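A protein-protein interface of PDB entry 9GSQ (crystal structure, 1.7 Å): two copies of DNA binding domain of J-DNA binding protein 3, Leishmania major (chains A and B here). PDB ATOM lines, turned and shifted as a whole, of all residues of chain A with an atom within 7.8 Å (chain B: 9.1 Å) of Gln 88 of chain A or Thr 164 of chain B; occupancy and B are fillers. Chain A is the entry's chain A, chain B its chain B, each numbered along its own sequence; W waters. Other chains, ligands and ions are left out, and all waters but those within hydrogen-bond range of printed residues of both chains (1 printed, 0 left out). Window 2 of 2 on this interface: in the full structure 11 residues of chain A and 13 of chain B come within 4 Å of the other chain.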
ATOM      1  N   GLN A  76      -9.299  21.995  26.673  1.00  0.00           N
ATOM      2  CA  GLN A  76      -9.420  21.048  25.580  1.00  0.00           C
ATOM      3  C   GLN A  76     -10.882  20.704  25.296  1.00  0.00           C
ATOM      4  O   GLN A  76     -11.265  20.556  24.137  1.00  0.00           O
ATOM      5  CB  GLN A  76      -8.599  19.779  25.887  1.00  0.00           C
ATOM      6  CG  GLN A  76      -7.122  20.058  25.872  1.00  0.00           C
ATOM      7  CD  GLN A  76      -6.305  18.813  26.152  1.00  0.00           C
ATOM      8  OE1 GLN A  76      -6.736  17.690  25.894  1.00  0.00           O
ATOM      9  NE2 GLN A  76      -5.117  19.021  26.668  1.00  0.00           N
ATOM     10  N   ALA A  80     -12.789  21.454  21.813  1.00  0.00           N
ATOM     11  CA  ALA A  80     -13.499  20.421  21.078  1.00  0.00           C
ATOM     12  C   ALA A  80     -14.914  20.882  20.740  1.00  0.00           C
ATOM     13  O   ALA A  80     -15.333  20.782  19.585  1.00  0.00           O
ATOM     14  CB  ALA A  80     -13.531  19.110  21.857  1.00  0.00           C
ATOM     15  N   GLY A  84     -17.130  21.516  17.093  1.00  0.00           N
ATOM     16  CA  GLY A  84     -18.200  20.577  16.783  1.00  0.00           C
ATOM     17  C   GLY A  84     -17.838  19.097  16.893  1.00  0.00           C
ATOM     18  O   GLY A  84     -18.423  18.254  16.212  1.00  0.00           O
ATOM     19  N   ARG A  85     -16.878  18.782  17.771  1.00  0.00           N
ATOM     20  CA  ARG A  85     -16.433  17.411  17.953  1.00  0.00           C
ATOM     21  C   ARG A  85     -16.481  17.034  19.431  1.00  0.00           C
ATOM     22  O   ARG A  85     -16.264  17.871  20.306  1.00  0.00           O
ATOM     23  CB  ARG A  85     -15.023  17.201  17.368  1.00  0.00           C
ATOM     24  CG  ARG A  85     -14.026  18.279  17.759  1.00  0.00           C
ATOM     25  CD  ARG A  85     -12.583  17.898  17.515  1.00  0.00           C
ATOM     26  NE  ARG A  85     -11.684  18.885  18.103  1.00  0.00           N
ATOM     27  CZ  ARG A  85     -10.361  18.788  18.128  1.00  0.00           C
ATOM     28  NH1 ARG A  85      -9.720  17.890  17.398  1.00  0.00           N
ATOM     29  NH2 ARG A  85      -9.664  19.628  18.890  1.00  0.00           N
ATOM     30  N   ALA A  86     -16.799  15.764  19.696  1.00  0.00           N
ATOM     31  CA  ALA A  86     -16.725  15.218  21.040  1.00  0.00           C
ATOM     32  C   ALA A  86     -15.259  14.935  21.356  1.00  0.00           C
ATOM     33  O   ALA A  86     -14.568  14.295  20.565  1.00  0.00           O
ATOM     34  CB  ALA A  86     -17.552  13.952  21.159  1.00  0.00           C
ATOM     35  N   MET A  87     -14.789  15.457  22.492  1.00  0.00           N
ATOM     36  CA  MET A  87     -13.415  15.251  22.908  1.00  0.00           C
ATOM     37  C   MET A  87     -13.231  13.766  23.222  1.00  0.00           C
ATOM     38  O   MET A  87     -13.947  13.219  24.055  1.00  0.00           O
ATOM     39  CB  MET A  87     -13.111  16.142  24.109  1.00  0.00           C
ATOM     40  CG  MET A  87     -11.818  15.834  24.773  1.00  0.00           C
ATOM     41  SD  MET A  87     -11.557  16.950  26.153  1.00  0.00           S
ATOM     42  CE  MET A  87     -10.022  16.363  26.699  1.00  0.00           C
ATOM     43  N   GLN A  88     -12.282  13.141  22.520  1.00  0.00           N
ATOM     44  CA  GLN A  88     -12.044  11.705  22.546  1.00  0.00           C
ATOM     45  C   GLN A  88     -11.029  11.262  23.599  1.00  0.00           C
ATOM     46  O   GLN A  88     -11.171  10.205  24.204  1.00  0.00           O
ATOM     47  CB  GLN A  88     -11.504  11.262  21.167  1.00  0.00           C
ATOM     48  CG  GLN A  88     -10.348  12.162  20.619  1.00  0.00           C
ATOM     49  CD  GLN A  88      -9.402  11.457  19.688  1.00  0.00           C
ATOM     50  OE1 GLN A  88      -8.952  10.351  19.962  1.00  0.00           O
ATOM     51  NE2 GLN A  88      -9.061  12.081  18.574  1.00  0.00           N
ATOM     52  N   ARG A  89      -9.976  12.064  23.776  1.00  0.00           N
ATOM     53  CA  ARG A  89      -8.894  11.745  24.691  1.00  0.00           C
ATOM     54  C   ARG A  89      -8.326  13.082  25.150  1.00  0.00           C
ATOM     55  O   ARG A  89      -8.328  14.048  24.398  1.00  0.00           O
ATOM     56  CB  ARG A  89      -7.741  10.939  24.049  1.00  0.00           C
ATOM     57  CG  ARG A  89      -8.094   9.583  23.492  1.00  0.00           C
ATOM     58  CD  ARG A  89      -6.938   9.040  22.637  1.00  0.00           C
ATOM     59  NE  ARG A  89      -6.799   9.782  21.387  1.00  0.00           N
ATOM     60  CZ  ARG A  89      -5.730   9.744  20.596  1.00  0.00           C
ATOM     61  NH1 ARG A  89      -4.611   9.140  20.968  1.00  0.00           N
ATOM     62  NH2 ARG A  89      -5.771  10.363  19.420  1.00  0.00           N
ATOM     63  N   PHE A  90      -7.862  13.109  26.396  1.00  0.00           N
ATOM     64  CA  PHE A  90      -7.071  14.211  26.906  1.00  0.00           C
ATOM     65  C   PHE A  90      -5.682  14.166  26.280  1.00  0.00           C
ATOM     66  O   PHE A  90      -5.057  13.105  26.232  1.00  0.00           O
ATOM     67  CB  PHE A  90      -6.951  14.100  28.428  1.00  0.00           C
ATOM     68  CG  PHE A  90      -6.144  15.175  29.100  1.00  0.00           C
ATOM     69  CD1 PHE A  90      -6.710  16.384  29.423  1.00  0.00           C
ATOM     70  CD2 PHE A  90      -4.821  14.973  29.411  1.00  0.00           C
ATOM     71  CE1 PHE A  90      -5.964  17.380  30.047  1.00  0.00           C
ATOM     72  CE2 PHE A  90      -4.075  15.970  30.045  1.00  0.00           C
ATOM     73  CZ  PHE A  90      -4.644  17.167  30.347  1.00  0.00           C
ATOM     74  N   THR A  91      -5.194  15.336  25.845  1.00  0.00           N
ATOM     75  CA  THR A  91      -3.833  15.468  25.339  1.00  0.00           C
ATOM     76  C   THR A  91      -2.887  15.936  26.444  1.00  0.00           C
ATOM     77  O   THR A  91      -3.042  17.030  26.989  1.00  0.00           O
ATOM     78  CB  THR A  91      -3.756  16.457  24.196  1.00  0.00           C
ATOM     79  OG1 THR A  91      -4.636  16.034  23.169  1.00  0.00           O
ATOM     80  CG2 THR A  91      -2.359  16.609  23.654  1.00  0.00           C
ATOM     81  N   GLU A 144     -11.562   9.063  33.545  1.00  0.00           N
ATOM     82  CA  GLU A 144     -10.531   8.134  33.119  1.00  0.00           C
ATOM     83  C   GLU A 144     -10.658   7.690  31.670  1.00  0.00           C
ATOM     84  O   GLU A 144      -9.661   7.302  31.077  1.00  0.00           O
ATOM     85  CB  GLU A 144     -10.498   6.917  34.022  1.00  0.00           C
ATOM     86  CG  GLU A 144      -9.786   7.184  35.318  1.00  0.00           C
ATOM     87  CD  GLU A 144     -10.072   6.120  36.361  1.00  0.00           C
ATOM     88  OE1 GLU A 144     -11.115   6.251  37.047  1.00  0.00           O
ATOM     89  OE2 GLU A 144      -9.291   5.147  36.445  1.00  0.00           O
ATOM     90  N   THR A 145     -11.860   7.785  31.087  1.00  0.00           N
ATOM     91  CA  THR A 145     -11.973   7.562  29.649  1.00  0.00           C
ATOM     92  C   THR A 145     -11.232   8.625  28.843  1.00  0.00           C
ATOM     93  O   THR A 145     -10.885   8.380  27.690  1.00  0.00           O
ATOM     94  CB  THR A 145     -13.414   7.454  29.181  1.00  0.00           C
ATOM     95  OG1 THR A 145     -14.116   8.620  29.554  1.00  0.00           O
ATOM     96  CG2 THR A 145     -14.100   6.226  29.753  1.00  0.00           C
ATOM     97  N   MET A 146     -11.008   9.792  29.451  1.00  0.00           N
ATOM     98  CA  MET A 146     -10.279  10.874  28.803  1.00  0.00           C
ATOM     99  C   MET A 146      -8.799  10.834  29.162  1.00  0.00           C
ATOM    100  O   MET A 146      -7.938  11.010  28.306  1.00  0.00           O
ATOM    101  CB  MET A 146     -10.858  12.238  29.214  1.00  0.00           C
ATOM    102  CG  MET A 146     -12.241  12.503  28.754  1.00  0.00           C
ATOM    103  SD  MET A 146     -12.291  12.735  26.994  1.00  0.00           S
ATOM    104  CE  MET A 146     -12.949  11.139  26.494  1.00  0.00           C
ATOM    105  N   LEU A 147      -8.509  10.604  30.443  1.00  0.00           N
ATOM    106  CA  LEU A 147      -7.146  10.515  30.920  1.00  0.00           C
ATOM    107  C   LEU A 147      -7.046   9.294  31.822  1.00  0.00           C
ATOM    108  O   LEU A 147      -7.487   9.324  32.975  1.00  0.00           O
ATOM    109  CB  LEU A 147      -6.753  11.806  31.642  1.00  0.00           C
ATOM    110  CG  LEU A 147      -5.407  11.797  32.380  1.00  0.00           C
ATOM    111  CD1 LEU A 147      -4.304  11.398  31.461  1.00  0.00           C
ATOM    112  CD2 LEU A 147      -5.097  13.161  32.941  1.00  0.00           C
ATOM    113  N   LYS B 110     -19.769   3.668  29.631  1.00  0.00           N
ATOM    114  CA  LYS B 110     -18.713   4.680  29.668  1.00  0.00           C
ATOM    115  C   LYS B 110     -18.870   5.576  30.886  1.00  0.00           C
ATOM    116  O   LYS B 110     -17.921   5.775  31.641  1.00  0.00           O
ATOM    117  CB  LYS B 110     -18.718   5.505  28.379  1.00  0.00           C
ATOM    118  CG  LYS B 110     -17.661   6.582  28.313  1.00  0.00           C
ATOM    119  CD  LYS B 110     -17.576   7.225  26.930  1.00  0.00           C
ATOM    120  CE  LYS B 110     -16.440   8.229  26.879  1.00  0.00           C
ATOM    121  NZ  LYS B 110     -16.208   8.768  25.519  1.00  0.00           N
ATOM    122  N   ASP B 114     -16.367   5.770  34.295  1.00  0.00           N
ATOM    123  CA  ASP B 114     -15.775   7.003  34.781  1.00  0.00           C
ATOM    124  C   ASP B 114     -16.178   7.307  36.225  1.00  0.00           C
ATOM    125  O   ASP B 114     -15.427   7.964  36.934  1.00  0.00           O
ATOM    126  CB  ASP B 114     -16.125   8.145  33.844  1.00  0.00           C
ATOM    127  CG  ASP B 114     -15.274   8.115  32.600  1.00  0.00           C
ATOM    128  OD1 ASP B 114     -14.126   7.603  32.685  1.00  0.00           O
ATOM    129  OD2 ASP B 114     -15.765   8.561  31.518  1.00  0.00           O
ATOM    130  N   TRP B 125     -10.104   0.698  30.649  1.00  0.00           N
ATOM    131  CA  TRP B 125     -11.329   0.828  29.864  1.00  0.00           C
ATOM    132  C   TRP B 125     -11.560  -0.307  28.859  1.00  0.00           C
ATOM    133  O   TRP B 125     -12.653  -0.888  28.808  1.00  0.00           O
ATOM    134  CB  TRP B 125     -11.304   2.172  29.121  1.00  0.00           C
ATOM    135  CG  TRP B 125     -12.351   2.299  28.065  1.00  0.00           C
ATOM    136  CD1 TRP B 125     -12.151   2.373  26.721  1.00  0.00           C
ATOM    137  CD2 TRP B 125     -13.779   2.297  28.263  1.00  0.00           C
ATOM    138  NE1 TRP B 125     -13.361   2.427  26.064  1.00  0.00           N
ATOM    139  CE2 TRP B 125     -14.376   2.414  26.992  1.00  0.00           C
ATOM    140  CE3 TRP B 125     -14.603   2.248  29.394  1.00  0.00           C
ATOM    141  CZ2 TRP B 125     -15.753   2.449  26.811  1.00  0.00           C
ATOM    142  CZ3 TRP B 125     -15.970   2.273  29.218  1.00  0.00           C
ATOM    143  CH2 TRP B 125     -16.536   2.397  27.943  1.00  0.00           C
ATOM    144  N   TYR B 156     -19.763  -2.326  18.726  1.00  0.00           N
ATOM    145  CA  TYR B 156     -19.089  -1.428  19.641  1.00  0.00           C
ATOM    146  C   TYR B 156     -18.191  -0.471  18.855  1.00  0.00           C
ATOM    147  O   TYR B 156     -18.188   0.740  19.082  1.00  0.00           O
ATOM    148  CB  TYR B 156     -18.323  -2.226  20.692  1.00  0.00           C
ATOM    149  CG  TYR B 156     -17.383  -1.351  21.472  1.00  0.00           C
ATOM    150  CD1 TYR B 156     -17.850  -0.505  22.461  1.00  0.00           C
ATOM    151  CD2 TYR B 156     -16.041  -1.291  21.146  1.00  0.00           C
ATOM    152  CE1 TYR B 156     -16.991   0.338  23.143  1.00  0.00           C
ATOM    153  CE2 TYR B 156     -15.178  -0.452  21.816  1.00  0.00           C
ATOM    154  CZ  TYR B 156     -15.653   0.351  22.828  1.00  0.00           C
ATOM    155  OH  TYR B 156     -14.782   1.186  23.473  1.00  0.00           O
ATOM    156  N   MET B 157     -17.451  -1.014  17.889  1.00  0.00           N
ATOM    157  CA  MET B 157     -16.578  -0.198  17.064  1.00  0.00           C
ATOM    158  C   MET B 157     -17.381   0.836  16.275  1.00  0.00           C
ATOM    159  O   MET B 157     -16.947   1.983  16.136  1.00  0.00           O
ATOM    160  CB  MET B 157     -15.748  -1.092  16.122  1.00  0.00           C
ATOM    161  CG  MET B 157     -14.215  -1.042  16.392  1.00  0.00           C
ATOM    162  SD  MET B 157     -13.748  -1.165  18.132  1.00  0.00           S
ATOM    163  CE  MET B 157     -12.773   0.293  18.293  1.00  0.00           C
ATOM    164  N   ASP B 158     -18.553   0.429  15.772  1.00  0.00           N
ATOM    165  CA  ASP B 158     -19.449   1.351  15.093  1.00  0.00           C
ATOM    166  C   ASP B 158     -19.870   2.501  16.003  1.00  0.00           C
ATOM    167  O   ASP B 158     -19.967   3.645  15.558  1.00  0.00           O
ATOM    168  CB  ASP B 158     -20.709   0.662  14.597  1.00  0.00           C
ATOM    169  CG  ASP B 158     -20.511  -0.304  13.453  1.00  0.00           C
ATOM    170  OD1 ASP B 158     -19.442  -0.248  12.813  1.00  0.00           O
ATOM    171  OD2 ASP B 158     -21.413  -1.155  13.230  1.00  0.00           O
ATOM    172  N   TRP B 159     -20.123   2.196  17.282  1.00  0.00           N
ATOM    173  CA  TRP B 159     -20.484   3.216  18.256  1.00  0.00           C
ATOM    174  C   TRP B 159     -19.302   4.138  18.554  1.00  0.00           C
ATOM    175  O   TRP B 159     -19.462   5.347  18.630  1.00  0.00           O
ATOM    176  CB  TRP B 159     -21.012   2.559  19.546  1.00  0.00           C
ATOM    177  CG  TRP B 159     -21.204   3.478  20.706  1.00  0.00           C
ATOM    178  CD1 TRP B 159     -22.281   4.279  20.964  1.00  0.00           C
ATOM    179  CD2 TRP B 159     -20.274   3.713  21.753  1.00  0.00           C
ATOM    180  NE1 TRP B 159     -22.089   4.967  22.128  1.00  0.00           N
ATOM    181  CE2 TRP B 159     -20.854   4.658  22.626  1.00  0.00           C
ATOM    182  CE3 TRP B 159     -19.012   3.205  22.059  1.00  0.00           C
ATOM    183  CZ2 TRP B 159     -20.219   5.090  23.776  1.00  0.00           C
ATOM    184  CZ3 TRP B 159     -18.388   3.635  23.214  1.00  0.00           C
ATOM    185  CH2 TRP B 159     -18.999   4.565  24.058  1.00  0.00           C
ATOM    186  N   VAL B 160     -18.105   3.563  18.714  1.00  0.00           N
ATOM    187  CA  VAL B 160     -16.907   4.369  18.908  1.00  0.00           C
ATOM    188  C   VAL B 160     -16.731   5.361  17.754  1.00  0.00           C
ATOM    189  O   VAL B 160     -16.454   6.541  17.982  1.00  0.00           O
ATOM    190  CB  VAL B 160     -15.641   3.496  19.079  1.00  0.00           C
ATOM    191  CG1 VAL B 160     -14.373   4.354  19.041  1.00  0.00           C
ATOM    192  CG2 VAL B 160     -15.692   2.664  20.364  1.00  0.00           C
ATOM    193  N   LYS B 161     -16.920   4.874  16.520  1.00  0.00           N
ATOM    194  CA  LYS B 161     -16.741   5.692  15.326  1.00  0.00           C
ATOM    195  C   LYS B 161     -17.778   6.803  15.186  1.00  0.00           C
ATOM    196  O   LYS B 161     -17.450   7.906  14.761  1.00  0.00           O
ATOM    197  CB  LYS B 161     -16.767   4.820  14.065  1.00  0.00           C
ATOM    198  CG  LYS B 161     -15.479   4.009  13.902  1.00  0.00           C
ATOM    199  CD  LYS B 161     -15.476   3.075  12.702  1.00  0.00           C
ATOM    200  CE  LYS B 161     -14.264   2.177  12.711  1.00  0.00           C
ATOM    201  NZ  LYS B 161     -14.308   1.169  11.616  1.00  0.00           N
ATOM    202  N   GLY B 162     -19.032   6.496  15.530  1.00  0.00           N
ATOM    203  CA  GLY B 162     -20.123   7.451  15.426  1.00  0.00           C
ATOM    204  C   GLY B 162     -19.984   8.663  16.346  1.00  0.00           C
ATOM    205  O   GLY B 162     -20.567   9.711  16.079  1.00  0.00           O
ATOM    206  N   GLY B 163     -19.217   8.507  17.435  1.00  0.00           N
ATOM    207  CA  GLY B 163     -19.019   9.585  18.391  1.00  0.00           C
ATOM    208  C   GLY B 163     -17.933  10.565  17.950  1.00  0.00           C
ATOM    209  O   GLY B 163     -18.156  11.774  17.902  1.00  0.00           O
ATOM    210  N   THR B 164     -16.756  10.015  17.639  1.00  0.00           N
ATOM    211  CA  THR B 164     -15.615  10.804  17.203  1.00  0.00           C
ATOM    212  C   THR B 164     -15.779  11.224  15.747  1.00  0.00           C
ATOM    213  O   THR B 164     -15.750  10.379  14.857  1.00  0.00           O
ATOM    214  CB  THR B 164     -14.316  10.017  17.444  1.00  0.00           C
ATOM    215  OG1 THR B 164     -14.457   8.692  16.924  1.00  0.00           O
ATOM    216  CG2 THR B 164     -13.967   9.922  18.923  1.00  0.00           C
ATOM    217  N   VAL B 180     -26.647  11.428  21.729  1.00  0.00           N
ATOM    218  CA  VAL B 180     -26.415  11.071  23.119  1.00  0.00           C
ATOM    219  C   VAL B 180     -27.516  11.619  24.025  1.00  0.00           C
ATOM    220  O   VAL B 180     -28.019  10.906  24.881  1.00  0.00           O
ATOM    221  CB  VAL B 180     -25.030  11.553  23.597  1.00  0.00           C
ATOM    222  CG1 VAL B 180     -24.865  11.375  25.106  1.00  0.00           C
ATOM    223  CG2 VAL B 180     -23.910  10.848  22.838  1.00  0.00           C
HETATM  224  O   HOH W   1     -12.894   8.320  36.313  1.00  0.00           O
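Of the 14 printed residues of chain A, 4 touch a printed residue of chain B. Printed residues of chain A that touch a printed residue of chain B: Ala 86, Gln 88, Glu 144 and Thr 145.
Of the printed residues of chain B, Ala 86 of chain A touches Gly 163 (3.96 Å). Gln 88 of chain A touches one residue of chain B. No residue of chain B comes within 4 Å of Arg 89 of chain A. Of the printed residues of chain B, Thr 145 of chain A touches Lys 110 and Asp 114. Printed residues of chain A within 4 Å of Thr 164 of chain B: Gln 88 (3.6 Å). The nearest residue of chain B that does not touch Gln 88 of chain A is Lys 110 of chain B (5.4 Å). The nearest residue of chain A that does not touch Thr 164 of chain B is Ala 86 of chain A (4.7 Å).
Among the printed residues, pairs that only touch across the chains: Ala 86 of chain A with Gly 163 of chain B (3.96 Å), Gln 88 of chain A with Thr 164 of chain B (3.6 Å) and Thr 145 of chain A with Lys 110 of chain B (3.6 Å).
The side-chain carboxylate (OD1) of Asp 114 of chain B is in hydrogen-bond range of the backbone NH (N) of Glu 144 of chain A, 3.1 Å away. The side-chain hydroxyl of Thr 145 of chain A sits at hydrogen-bond distance from the side-chain carboxylate of Asp 114 of chain B (2.6 Å).
No position is printed for both chains. Of the 5 pairs that touch across the chains among the printed residues, none has its exchanged pair printed and touching as well.
Water W1 bridges the backbone carbonyl oxygen of Asp 114 of chain B (2.6 Å) and the side-chain carboxylate of Glu 144 of chain A (2.8 Å).
The guanidinium group (NE) of Arg 89 of chain A sits at hydrogen-bond distance from the side-chain amide oxygen (OE1) of Gln 88 of chain A. O of Val 160 of chain B lies within hydrogen-bond range of OG1 of Thr 164 of chain B, at 3.1 Å.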
